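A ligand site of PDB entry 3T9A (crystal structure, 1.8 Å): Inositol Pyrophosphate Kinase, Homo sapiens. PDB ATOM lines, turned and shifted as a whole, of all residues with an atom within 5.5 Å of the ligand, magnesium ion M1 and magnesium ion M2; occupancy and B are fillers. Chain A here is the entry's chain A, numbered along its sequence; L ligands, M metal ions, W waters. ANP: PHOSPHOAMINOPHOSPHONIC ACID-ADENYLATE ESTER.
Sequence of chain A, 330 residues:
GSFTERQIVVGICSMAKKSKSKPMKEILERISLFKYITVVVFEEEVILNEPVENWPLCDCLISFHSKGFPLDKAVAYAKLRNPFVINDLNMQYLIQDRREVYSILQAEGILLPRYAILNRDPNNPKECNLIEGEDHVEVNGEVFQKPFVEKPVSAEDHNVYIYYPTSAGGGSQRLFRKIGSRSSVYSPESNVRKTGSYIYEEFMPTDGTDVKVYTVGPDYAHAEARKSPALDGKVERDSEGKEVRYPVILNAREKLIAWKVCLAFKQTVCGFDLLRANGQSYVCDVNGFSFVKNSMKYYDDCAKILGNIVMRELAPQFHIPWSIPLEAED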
ATOM      1  N   ARG A  98      14.616  15.781  13.350  1.00  0.00           N
ATOM      2  CA  ARG A  98      14.455  17.102  12.739  1.00  0.00           C
ATOM      3  C   ARG A  98      15.033  18.222  13.599  1.00  0.00           C
ATOM      4  O   ARG A  98      15.545  19.201  13.097  1.00  0.00           O
ATOM      5  CB  ARG A  98      12.975  17.378  12.444  1.00  0.00           C
ATOM      6  CG  ARG A  98      12.376  16.497  11.348  1.00  0.00           C
ATOM      7  CD  ARG A  98      10.968  16.972  11.010  1.00  0.00           C
ATOM      8  NE  ARG A  98      10.162  15.907  10.424  1.00  0.00           N
ATOM      9  CZ  ARG A  98      10.108  15.624   9.118  1.00  0.00           C
ATOM     10  NH1 ARG A  98      10.826  16.322   8.237  1.00  0.00           N
ATOM     11  NH2 ARG A  98       9.355  14.619   8.706  1.00  0.00           N
ATOM     12  N   TYR A 102      17.883  20.814  12.126  1.00  0.00           N
ATOM     13  CA  TYR A 102      17.735  22.273  12.152  1.00  0.00           C
ATOM     14  C   TYR A 102      18.863  22.947  12.944  1.00  0.00           C
ATOM     15  O   TYR A 102      19.368  23.987  12.537  1.00  0.00           O
ATOM     16  CB  TYR A 102      16.347  22.687  12.661  1.00  0.00           C
ATOM     17  CG  TYR A 102      15.310  22.759  11.550  1.00  0.00           C
ATOM     18  CD1 TYR A 102      15.477  22.048  10.361  1.00  0.00           C
ATOM     19  CD2 TYR A 102      14.174  23.552  11.688  1.00  0.00           C
ATOM     20  CE1 TYR A 102      14.551  22.131   9.324  1.00  0.00           C
ATOM     21  CE2 TYR A 102      13.223  23.640  10.666  1.00  0.00           C
ATOM     22  CZ  TYR A 102      13.423  22.926   9.491  1.00  0.00           C
ATOM     23  OH  TYR A 102      12.508  23.006   8.462  1.00  0.00           O
ATOM     24  N   PRO A 113      13.336  28.047   7.643  1.00  0.00           N
ATOM     25  CA  PRO A 113      12.139  28.737   8.143  1.00  0.00           C
ATOM     26  C   PRO A 113      12.274  29.068   9.630  1.00  0.00           C
ATOM     27  O   PRO A 113      12.884  28.304  10.381  1.00  0.00           O
ATOM     28  CB  PRO A 113      11.025  27.699   7.919  1.00  0.00           C
ATOM     29  CG  PRO A 113      11.519  26.844   6.772  1.00  0.00           C
ATOM     30  CD  PRO A 113      13.004  26.716   7.067  1.00  0.00           C
ATOM     31  N   VAL A 149       3.452  25.226   9.647  1.00  0.00           N
ATOM     32  CA  VAL A 149       3.711  23.817   9.349  1.00  0.00           C
ATOM     33  C   VAL A 149       4.047  23.107  10.657  1.00  0.00           C
ATOM     34  O   VAL A 149       4.720  23.669  11.532  1.00  0.00           O
ATOM     35  CB  VAL A 149       4.847  23.662   8.269  1.00  0.00           C
ATOM     36  CG1 VAL A 149       5.038  22.194   7.832  1.00  0.00           C
ATOM     37  CG2 VAL A 149       4.544  24.520   7.041  1.00  0.00           C
ATOM     38  N   LYS A 151       5.659  19.551  12.051  1.00  0.00           N
ATOM     39  CA  LYS A 151       6.394  18.340  11.633  1.00  0.00           C
ATOM     40  C   LYS A 151       6.715  17.492  12.834  1.00  0.00           C
ATOM     41  O   LYS A 151       7.203  18.018  13.844  1.00  0.00           O
ATOM     42  CB  LYS A 151       7.685  18.700  10.888  1.00  0.00           C
ATOM     43  CG  LYS A 151       7.499  19.641   9.689  1.00  0.00           C
ATOM     44  CD  LYS A 151       8.860  19.926   9.020  1.00  0.00           C
ATOM     45  CE  LYS A 151       8.705  20.915   7.887  1.00  0.00           C
ATOM     46  NZ  LYS A 151       9.971  21.075   7.096  1.00  0.00           N
ATOM     47  N   ALA A 155      12.292  12.592  11.814  1.00  0.00           N
ATOM     48  CA  ALA A 155      12.425  12.796  10.362  1.00  0.00           C
ATOM     49  C   ALA A 155      11.896  11.634   9.528  1.00  0.00           C
ATOM     50  O   ALA A 155      11.594  11.816   8.349  1.00  0.00           O
ATOM     51  CB  ALA A 155      13.879  13.112  10.001  1.00  0.00           C
ATOM     52  N   ASP A 157       9.100  10.203  10.145  1.00  0.00           N
ATOM     53  CA  ASP A 157       7.647  10.320  10.211  1.00  0.00           C
ATOM     54  C   ASP A 157       7.243  11.400   9.234  1.00  0.00           C
ATOM     55  O   ASP A 157       7.457  12.606   9.489  1.00  0.00           O
ATOM     56  CB  ASP A 157       7.210  10.681  11.645  1.00  0.00           C
ATOM     57  CG  ASP A 157       5.696  10.669  11.823  1.00  0.00           C
ATOM     58  OD1 ASP A 157       4.955  10.848  10.845  1.00  0.00           O
ATOM     59  OD2 ASP A 157       5.242  10.516  12.987  1.00  0.00           O
ATOM     60  N   HIS A 158       6.619  10.982   8.135  1.00  0.00           N
ATOM     61  CA  HIS A 158       6.272  11.906   7.065  1.00  0.00           C
ATOM     62  C   HIS A 158       4.883  12.551   7.189  1.00  0.00           C
ATOM     63  O   HIS A 158       4.386  13.164   6.241  1.00  0.00           O
ATOM     64  CB  HIS A 158       6.466  11.198   5.720  1.00  0.00           C
ATOM     65  CG  HIS A 158       7.860  10.679   5.561  1.00  0.00           C
ATOM     66  ND1 HIS A 158       8.964  11.503   5.524  1.00  0.00           N
ATOM     67  CD2 HIS A 158       8.334   9.409   5.474  1.00  0.00           C
ATOM     68  CE1 HIS A 158      10.055  10.768   5.402  1.00  0.00           C
ATOM     69  NE2 HIS A 158       9.703   9.504   5.361  1.00  0.00           N
ATOM     70  N   ASN A 159       4.281  12.414   8.365  1.00  0.00           N
ATOM     71  CA  ASN A 159       2.958  12.987   8.629  1.00  0.00           C
ATOM     72  C   ASN A 159       3.079  14.462   9.031  1.00  0.00           C
ATOM     73  O   ASN A 159       2.904  14.820  10.187  1.00  0.00           O
ATOM     74  CB  ASN A 159       2.209  12.162   9.672  1.00  0.00           C
ATOM     75  CG  ASN A 159       1.894  10.782   9.158  1.00  0.00           C
ATOM     76  OD1 ASN A 159       1.146  10.629   8.183  1.00  0.00           O
ATOM     77  ND2 ASN A 159       2.492   9.768   9.761  1.00  0.00           N
ATOM     78  N   VAL A 160       3.410  15.275   8.041  1.00  0.00           N
ATOM     79  CA  VAL A 160       3.613  16.702   8.216  1.00  0.00           C
ATOM     80  C   VAL A 160       2.290  17.394   7.891  1.00  0.00           C
ATOM     81  O   VAL A 160       1.708  17.105   6.863  1.00  0.00           O
ATOM     82  CB  VAL A 160       4.706  17.204   7.248  1.00  0.00           C
ATOM     83  CG1 VAL A 160       4.730  18.731   7.161  1.00  0.00           C
ATOM     84  CG2 VAL A 160       6.095  16.636   7.631  1.00  0.00           C
ATOM     85  N   ILE A 162      -0.099  21.024   7.511  1.00  0.00           N
ATOM     86  CA  ILE A 162      -0.074  22.458   7.285  1.00  0.00           C
ATOM     87  C   ILE A 162      -1.455  22.970   7.700  1.00  0.00           C
ATOM     88  O   ILE A 162      -2.461  22.349   7.346  1.00  0.00           O
ATOM     89  CB  ILE A 162       0.256  22.766   5.793  1.00  0.00           C
ATOM     90  CG1 ILE A 162       1.640  22.213   5.440  1.00  0.00           C
ATOM     91  CG2 ILE A 162       0.217  24.282   5.528  1.00  0.00           C
ATOM     92  CD1 ILE A 162       1.965  22.182   3.987  1.00  0.00           C
ATOM     93  N   LEU A 175      -0.042  15.772   4.917  1.00  0.00           N
ATOM     94  CA  LEU A 175       0.879  15.118   3.995  1.00  0.00           C
ATOM     95  C   LEU A 175       1.280  13.744   4.538  1.00  0.00           C
ATOM     96  O   LEU A 175       1.194  13.479   5.747  1.00  0.00           O
ATOM     97  CB  LEU A 175       2.134  15.989   3.787  1.00  0.00           C
ATOM     98  CG  LEU A 175       2.046  17.353   3.073  1.00  0.00           C
ATOM     99  CD1 LEU A 175       0.973  18.300   3.568  1.00  0.00           C
ATOM    100  CD2 LEU A 175       3.414  18.017   3.190  1.00  0.00           C
ATOM    101  N   ARG A 177       3.736   9.844   3.212  1.00  0.00           N
ATOM    102  CA  ARG A 177       4.580   9.201   2.212  1.00  0.00           C
ATOM    103  C   ARG A 177       3.693   8.772   1.035  1.00  0.00           C
ATOM    104  O   ARG A 177       2.685   8.094   1.230  1.00  0.00           O
ATOM    105  CB  ARG A 177       5.366   8.040   2.846  1.00  0.00           C
ATOM    106  CG  ARG A 177       6.370   7.281   1.963  1.00  0.00           C
ATOM    107  CD  ARG A 177       7.204   8.130   0.987  1.00  0.00           C
ATOM    108  NE  ARG A 177       8.143   9.079   1.598  1.00  0.00           N
ATOM    109  CZ  ARG A 177       9.397   8.793   1.965  1.00  0.00           C
ATOM    110  NH1 ARG A 177       9.882   7.552   1.844  1.00  0.00           N
ATOM    111  NH2 ARG A 177      10.166   9.746   2.480  1.00  0.00           N
ATOM    112  N   GLU A 201       6.756  25.579  12.234  1.00  0.00           N
ATOM    113  CA  GLU A 201       7.484  26.538  11.424  1.00  0.00           C
ATOM    114  C   GLU A 201       6.612  27.430  10.561  1.00  0.00           C
ATOM    115  O   GLU A 201       5.487  27.052  10.175  1.00  0.00           O
ATOM    116  CB  GLU A 201       8.612  25.895  10.600  1.00  0.00           C
ATOM    117  CG  GLU A 201       8.209  24.836   9.634  1.00  0.00           C
ATOM    118  CD  GLU A 201       9.402  24.055   9.073  1.00  0.00           C
ATOM    119  OE1 GLU A 201       9.600  24.099   7.861  1.00  0.00           O
ATOM    120  OE2 GLU A 201      10.111  23.339   9.822  1.00  0.00           O
ATOM    121  N   GLU A 202       7.138  28.619  10.269  1.00  0.00           N
ATOM    122  CA  GLU A 202       6.486  29.555   9.385  1.00  0.00           C
ATOM    123  C   GLU A 202       6.381  28.927   7.995  1.00  0.00           C
ATOM    124  O   GLU A 202       7.336  28.297   7.515  1.00  0.00           O
ATOM    125  CB  GLU A 202       7.260  30.882   9.304  1.00  0.00           C
ATOM    126  CG  GLU A 202       8.635  30.782   8.650  1.00  0.00           C
ATOM    127  CD  GLU A 202       9.314  32.145   8.421  1.00  0.00           C
ATOM    128  OE1 GLU A 202       8.597  33.178   8.369  1.00  0.00           O
ATOM    129  OE2 GLU A 202      10.560  32.176   8.288  1.00  0.00           O
ATOM    130  N   PHE A 203       5.205  29.073   7.382  1.00  0.00           N
ATOM    131  CA  PHE A 203       4.993  28.597   6.026  1.00  0.00           C
ATOM    132  C   PHE A 203       5.642  29.534   5.001  1.00  0.00           C
ATOM    133  O   PHE A 203       5.348  30.744   4.990  1.00  0.00           O
ATOM    134  CB  PHE A 203       3.492  28.444   5.729  1.00  0.00           C
ATOM    135  CG  PHE A 203       3.194  27.943   4.349  1.00  0.00           C
ATOM    136  CD1 PHE A 203       2.966  28.838   3.295  1.00  0.00           C
ATOM    137  CD2 PHE A 203       3.177  26.573   4.090  1.00  0.00           C
ATOM    138  CE1 PHE A 203       2.723  28.377   2.025  1.00  0.00           C
ATOM    139  CE2 PHE A 203       2.909  26.094   2.811  1.00  0.00           C
ATOM    140  CZ  PHE A 203       2.680  26.988   1.771  1.00  0.00           C
ATOM    141  N   MET A 204       6.532  29.001   4.170  1.00  0.00           N
ATOM    142  CA  MET A 204       7.265  29.832   3.198  1.00  0.00           C
ATOM    143  C   MET A 204       6.521  29.842   1.871  1.00  0.00           C
ATOM    144  O   MET A 204       6.309  28.774   1.284  1.00  0.00           O
ATOM    145  CB  MET A 204       8.708  29.327   2.991  1.00  0.00           C
ATOM    146  CG  MET A 204       9.496  29.055   4.254  1.00  0.00           C
ATOM    147  SD  MET A 204       9.649  30.480   5.348  1.00  0.00           S
ATOM    148  CE  MET A 204      10.678  31.591   4.391  1.00  0.00           C
ATOM    149  N   PRO A 205       6.096  31.027   1.395  1.00  0.00           N
ATOM    150  CA  PRO A 205       5.409  31.105   0.102  1.00  0.00           C
ATOM    151  C   PRO A 205       6.333  30.847  -1.095  1.00  0.00           C
ATOM    152  O   PRO A 205       7.353  31.521  -1.255  1.00  0.00           O
ATOM    153  CB  PRO A 205       4.847  32.528   0.068  1.00  0.00           C
ATOM    154  CG  PRO A 205       5.656  33.301   1.049  1.00  0.00           C
ATOM    155  CD  PRO A 205       6.143  32.329   2.091  1.00  0.00           C
ATOM    156  N   ASP A 210       8.796  22.377  -5.008  1.00  0.00           N
ATOM    157  CA  ASP A 210       9.963  22.095  -4.175  1.00  0.00           C
ATOM    158  C   ASP A 210      11.175  21.917  -5.043  1.00  0.00           C
ATOM    159  O   ASP A 210      11.105  21.240  -6.066  1.00  0.00           O
ATOM    160  CB  ASP A 210       9.780  20.758  -3.438  1.00  0.00           C
ATOM    161  CG  ASP A 210       8.608  20.751  -2.508  1.00  0.00           C
ATOM    162  OD1 ASP A 210       8.266  21.835  -1.996  1.00  0.00           O
ATOM    163  OD2 ASP A 210       8.046  19.657  -2.269  1.00  0.00           O
ATOM    164  N   LYS A 212      14.520  19.959  -5.195  1.00  0.00           N
ATOM    165  CA  LYS A 212      15.208  18.807  -4.619  1.00  0.00           C
ATOM    166  C   LYS A 212      16.646  18.800  -5.083  1.00  0.00           C
ATOM    167  O   LYS A 212      16.920  18.813  -6.280  1.00  0.00           O
ATOM    168  CB  LYS A 212      14.538  17.525  -5.094  1.00  0.00           C
ATOM    169  CG  LYS A 212      13.049  17.656  -5.311  1.00  0.00           C
ATOM    170  CD  LYS A 212      12.294  17.459  -4.021  1.00  0.00           C
ATOM    171  CE  LYS A 212      12.424  16.015  -3.538  1.00  0.00           C
ATOM    172  NZ  LYS A 212      11.850  15.950  -2.180  1.00  0.00           N
ATOM    173  N   SER A 228       4.715  20.805  -5.023  1.00  0.00           N
ATOM    174  CA  SER A 228       4.589  20.635  -3.568  1.00  0.00           C
ATOM    175  C   SER A 228       3.300  19.911  -3.198  1.00  0.00           C
ATOM    176  O   SER A 228       2.255  20.186  -3.801  1.00  0.00           O
ATOM    177  CB  SER A 228       4.563  21.981  -2.844  1.00  0.00           C
ATOM    178  OG  SER A 228       4.295  21.772  -1.466  1.00  0.00           O
ATOM    179  N   PRO A 229       3.356  18.995  -2.205  1.00  0.00           N
ATOM    180  CA  PRO A 229       2.140  18.413  -1.612  1.00  0.00           C
ATOM    181  C   PRO A 229       1.357  19.368  -0.700  1.00  0.00           C
ATOM    182  O   PRO A 229       0.252  19.036  -0.261  1.00  0.00           O
ATOM    183  CB  PRO A 229       2.679  17.228  -0.794  1.00  0.00           C
ATOM    184  CG  PRO A 229       4.104  17.008  -1.220  1.00  0.00           C
ATOM    185  CD  PRO A 229       4.593  18.317  -1.775  1.00  0.00           C
ATOM    186  N   ALA A 230       1.907  20.540  -0.411  1.00  0.00           N
ATOM    187  CA  ALA A 230       1.345  21.506   0.550  1.00  0.00           C
ATOM    188  C   ALA A 230      -0.151  21.850   0.464  1.00  0.00           C
ATOM    189  O   ALA A 230      -0.838  21.860   1.498  1.00  0.00           O
ATOM    190  CB  ALA A 230       2.179  22.807   0.555  1.00  0.00           C
ATOM    191  N   ASP A 273      16.060  19.467   0.564  1.00  0.00           N
ATOM    192  CA  ASP A 273      15.024  20.240  -0.139  1.00  0.00           C
ATOM    193  C   ASP A 273      15.215  21.743   0.103  1.00  0.00           C
ATOM    194  O   ASP A 273      15.510  22.170   1.231  1.00  0.00           O
ATOM    195  CB  ASP A 273      13.632  19.836   0.346  1.00  0.00           C
ATOM    196  CG  ASP A 273      13.319  18.367   0.110  1.00  0.00           C
ATOM    197  OD1 ASP A 273      13.671  17.826  -0.960  1.00  0.00           O
ATOM    198  OD2 ASP A 273      12.711  17.744   0.997  1.00  0.00           O
ATOM    199  N   LEU A 275      13.253  25.593  -0.475  1.00  0.00           N
ATOM    200  CA  LEU A 275      12.077  26.375  -0.778  1.00  0.00           C
ATOM    201  C   LEU A 275      12.553  27.736  -1.274  1.00  0.00           C
ATOM    202  O   LEU A 275      13.175  28.489  -0.510  1.00  0.00           O
ATOM    203  CB  LEU A 275      11.230  26.569   0.489  1.00  0.00           C
ATOM    204  CG  LEU A 275      10.802  25.300   1.239  1.00  0.00           C
ATOM    205  CD1 LEU A 275      10.057  25.610   2.542  1.00  0.00           C
ATOM    206  CD2 LEU A 275       9.984  24.404   0.343  1.00  0.00           C
ATOM    207  N   CYS A 284      14.454  23.129   4.142  1.00  0.00           N
ATOM    208  CA  CYS A 284      13.386  22.677   5.064  1.00  0.00           C
ATOM    209  C   CYS A 284      13.558  21.214   5.512  1.00  0.00           C
ATOM    210  O   CYS A 284      12.854  20.772   6.428  1.00  0.00           O
ATOM    211  CB  CYS A 284      11.982  22.959   4.467  1.00  0.00           C
ATOM    212  SG  CYS A 284      11.575  21.936   3.006  1.00  0.00           S
ATOM    213  N   ASP A 285      14.486  20.481   4.891  1.00  0.00           N
ATOM    214  CA  ASP A 285      14.558  19.027   5.075  1.00  0.00           C
ATOM    215  C   ASP A 285      15.896  18.524   4.568  1.00  0.00           C
ATOM    216  O   ASP A 285      16.348  18.940   3.496  1.00  0.00           O
ATOM    217  CB  ASP A 285      13.437  18.398   4.208  1.00  0.00           C
ATOM    218  CG  ASP A 285      13.270  16.892   4.413  1.00  0.00           C
ATOM    219  OD1 ASP A 285      13.657  16.352   5.462  1.00  0.00           O
ATOM    220  OD2 ASP A 285      12.734  16.235   3.494  1.00  0.00           O
ATOM    221  N   VAL A 286      16.554  17.664   5.351  1.00  0.00           N
ATOM    222  CA  VAL A 286      17.855  17.101   4.988  1.00  0.00           C
ATOM    223  C   VAL A 286      17.676  15.578   5.135  1.00  0.00           C
ATOM    224  O   VAL A 286      17.416  15.086   6.235  1.00  0.00           O
ATOM    225  CB  VAL A 286      19.078  17.590   5.821  1.00  0.00           C
ATOM    226  CG1 VAL A 286      20.331  16.835   5.383  1.00  0.00           C
ATOM    227  CG2 VAL A 286      19.310  19.090   5.660  1.00  0.00           C
ATOM    228  N   ASN A 287      17.778  14.860   4.021  1.00  0.00           N
ATOM    229  CA  ASN A 287      17.439  13.434   3.971  1.00  0.00           C
ATOM    230  C   ASN A 287      18.594  12.442   4.007  1.00  0.00           C
ATOM    231  O   ASN A 287      18.353  11.229   4.169  1.00  0.00           O
ATOM    232  CB  ASN A 287      16.540  13.146   2.767  1.00  0.00           C
ATOM    233  CG  ASN A 287      15.175  13.785   2.905  1.00  0.00           C
ATOM    234  OD1 ASN A 287      14.569  13.750   3.981  1.00  0.00           O
ATOM    235  ND2 ASN A 287      14.656  14.334   1.811  1.00  0.00           N
HETATM  236  PG  ANP L   1      10.736  13.780   2.515  1.00  0.00           P
HETATM  237  O1G ANP L   1      11.471  14.743   1.514  1.00  0.00           O
HETATM  238  O2G ANP L   1      10.064  12.671   1.745  1.00  0.00           O
HETATM  239  O3G ANP L   1      11.817  13.189   3.491  1.00  0.00           O
HETATM  240  PB  ANP L   1       9.577  15.048   4.938  1.00  0.00           P
HETATM  241  O1B ANP L   1       8.550  14.225   5.628  1.00  0.00           O
HETATM  242  O2B ANP L   1      10.947  15.087   5.566  1.00  0.00           O
HETATM  243  N3B ANP L   1       9.591  14.706   3.340  1.00  0.00           N
HETATM  244  PA  ANP L   1       9.466  17.965   4.464  1.00  0.00           P
HETATM  245  O1A ANP L   1      10.118  18.661   5.572  1.00  0.00           O
HETATM  246  O2A ANP L   1      10.182  17.748   3.193  1.00  0.00           O
HETATM  247  O3A ANP L   1       8.879  16.526   5.010  1.00  0.00           O
HETATM  248  O5' ANP L   1       8.087  18.686   4.175  1.00  0.00           O
HETATM  249  C5' ANP L   1       7.296  18.115   3.113  1.00  0.00           C
HETATM  250  C4' ANP L   1       6.859  19.176   2.084  1.00  0.00           C
HETATM  251  O4' ANP L   1       6.015  20.125   2.747  1.00  0.00           O
HETATM  252  C3' ANP L   1       8.018  20.000   1.539  1.00  0.00           C
HETATM  253  O3' ANP L   1       8.551  19.312   0.430  1.00  0.00           O
HETATM  254  C2' ANP L   1       7.326  21.303   1.148  1.00  0.00           C
HETATM  255  O2' ANP L   1       6.581  21.170  -0.073  1.00  0.00           O
HETATM  256  C1' ANP L   1       6.359  21.484   2.312  1.00  0.00           C
HETATM  257  N9  ANP L   1       7.022  22.315   3.392  1.00  0.00           N
HETATM  258  C8  ANP L   1       7.815  21.754   4.492  1.00  0.00           C
HETATM  259  N7  ANP L   1       8.075  22.914   5.333  1.00  0.00           N
HETATM  260  C5  ANP L   1       7.590  23.998   4.715  1.00  0.00           C
HETATM  261  C6  ANP L   1       7.625  25.340   5.072  1.00  0.00           C
HETATM  262  N6  ANP L   1       8.214  25.734   6.205  1.00  0.00           N
HETATM  263  N1  ANP L   1       7.020  26.231   4.271  1.00  0.00           N
HETATM  264  C2  ANP L   1       6.430  25.867   3.140  1.00  0.00           C
HETATM  265  N3  ANP L   1       6.383  24.582   2.758  1.00  0.00           N
HETATM  266  C4  ANP L   1       6.948  23.630   3.540  1.00  0.00           C
HETATM  267 MG    MG M   1      12.722  14.329   4.828  1.00  0.00          MG
HETATM  268 MG    MG M   2      11.365  16.664   1.985  1.00  0.00          MG
HETATM  269  O   HOH W   1       8.243  15.049   0.212  1.00  0.00           O
HETATM  270  O   HOH W   2       5.916  14.822   4.595  1.00  0.00           O
HETATM  271  O   HOH W   3       9.950  16.988   0.533  1.00  0.00           O
HETATM  272  O   HOH W   4      11.923  13.889  -0.888  1.00  0.00           O
HETATM  273  O   HOH W   5       7.405  11.887   2.131  1.00  0.00           O
HETATM  274  O   HOH W   6       5.212  24.626   0.056  1.00  0.00           O
HETATM  275  O   HOH W   7      13.061  13.319   6.374  1.00  0.00           O
HETATM  276  O   HOH W   8      13.098  10.989   3.174  1.00  0.00           O
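Water W3 bridges an oxygen (O3') of the ligand (2.7 Å) and the side-chain amino group (NZ) of Lys 212 (3.5 Å). Water W4 lies within hydrogen-bond range of NZ of Lys 212 (2.4 Å) and O2G of the ligand (3.4 Å). Water W5 bridges an oxygen (O2G) of the ligand (2.8 Å) and the guanidinium group of Arg 177 (3.0 Å). Water W2 lies within hydrogen-bond range of O of His 158 and O1B of the ligand. Water W6 bridges N3 of the ligand (2.9 Å) and OG of Ser 228 (3.4 Å).
Two residues have an atom within 4 Å of magnesium ion M1: Asp 285 and Asn 287.
Two residues have an atom within 4 Å of magnesium ion M2: Asp 273 and Asp 285. Along chain A the residues within 4 Å of magnesium ion M2 span positions 273 to 285. The nearest printed residue that does not touch magnesium ion M2 is Asn 287 (4.04 Å).
Magnesium ion M2 is bound by O1G of the ligand, 2.0 Å away. OD2 of Asp 273 binds magnesium ion M2 (2.0 Å). Magnesium ion M2 is bound by O2A of the ligand (2.0 Å). Magnesium ion M2 is bound by water W3 (2.1 Å). Magnesium ion M2 is bound by OD2 of Asp 285, at 2.1 Å.
Pro 113 touches the ligand (CG to N6, 3.5 Å). CG2 of Val 149 touches C6 of the ligand, 3.7 Å away. Val 160 touches the ligand (CG2 to O3A, 3.8 Å). Leu 175 touches the ligand (CD2 to O4', 3.4 Å). Phe 203 touches the ligand (CD2 to C2, 3.5 Å). Pro 229 touches the ligand (CD to O2', 3.9 Å). Leu 275 touches the ligand. Cys 284 touches the ligand (O to O1A, 3.6 Å).
OD1 of Asp 210 sits at hydrogen-bond distance from O2' of the ligand, at 2.6 Å. The side-chain carboxylate (OE1) of Glu 201 lies within hydrogen-bond range of a nitrogen (N6) of the ligand. The side-chain hydroxyl of Ser 228 lies within hydrogen-bond range of an oxygen (O2') of the ligand (2.7 Å). ND1 of His 158 lies within hydrogen-bond range of O1B of the ligand, 2.8 Å away. The backbone NH (N) of Met 204 is in hydrogen-bond range of a nitrogen (N1) of the ligand (2.8 Å). The side-chain amino group of Lys 151 is in salt-bridge range of an oxygen (O1A) of the ligand, at 2.9 Å. NH2 of Arg 98 is in salt-bridge range of O1B of the ligand (3.2 Å). O of Glu 202 lies within hydrogen-bond range of N6 of the ligand (3.0 Å). An oxygen (O2G) of the ligand lies within salt-bridge range of the guanidinium group (NH2) of Arg 177. NZ of Lys 212 lies close to O1G of the ligand.
O of Asp 273 is in hydrogen-bond range of N of Cys 284 (3.2 Å). The side-chain carboxylate (OE1) of Glu 201 is in salt-bridge range of the side-chain amino group (NZ) of Lys 151. N of Val 149 lies within hydrogen-bond range of O of Glu 201. OH of Tyr 102 is in hydrogen-bond range of OE2 of Glu 201. OG of Ser 228 lies within hydrogen-bond range of N of Ala 230. The side-chain hydroxyl of Tyr 102 lies within hydrogen-bond range of the side-chain amino group of Lys 151. The backbone carbonyl oxygen (O) of Asp 157 lies within hydrogen-bond range of the guanidinium group (NH2) of Arg 98 (2.9 Å). The backbone NH of Leu 175 lies within hydrogen-bond range of the backbone carbonyl oxygen of Val 160, 2.9 Å away.
Magnesium ion M1 is bound by water W7 (1.9 Å), an oxygen (O3G) of the ligand (2.0 Å), an oxygen (O2B) of the ligand (2.1 Å), the side-chain amide oxygen (OD1) of Asn 287 (2.1 Å), the side-chain carboxylate (OD1) of Asp 285 (2.3 Å) and the side-chain carboxylate (OD2) of Asp 285 (2.3 Å).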
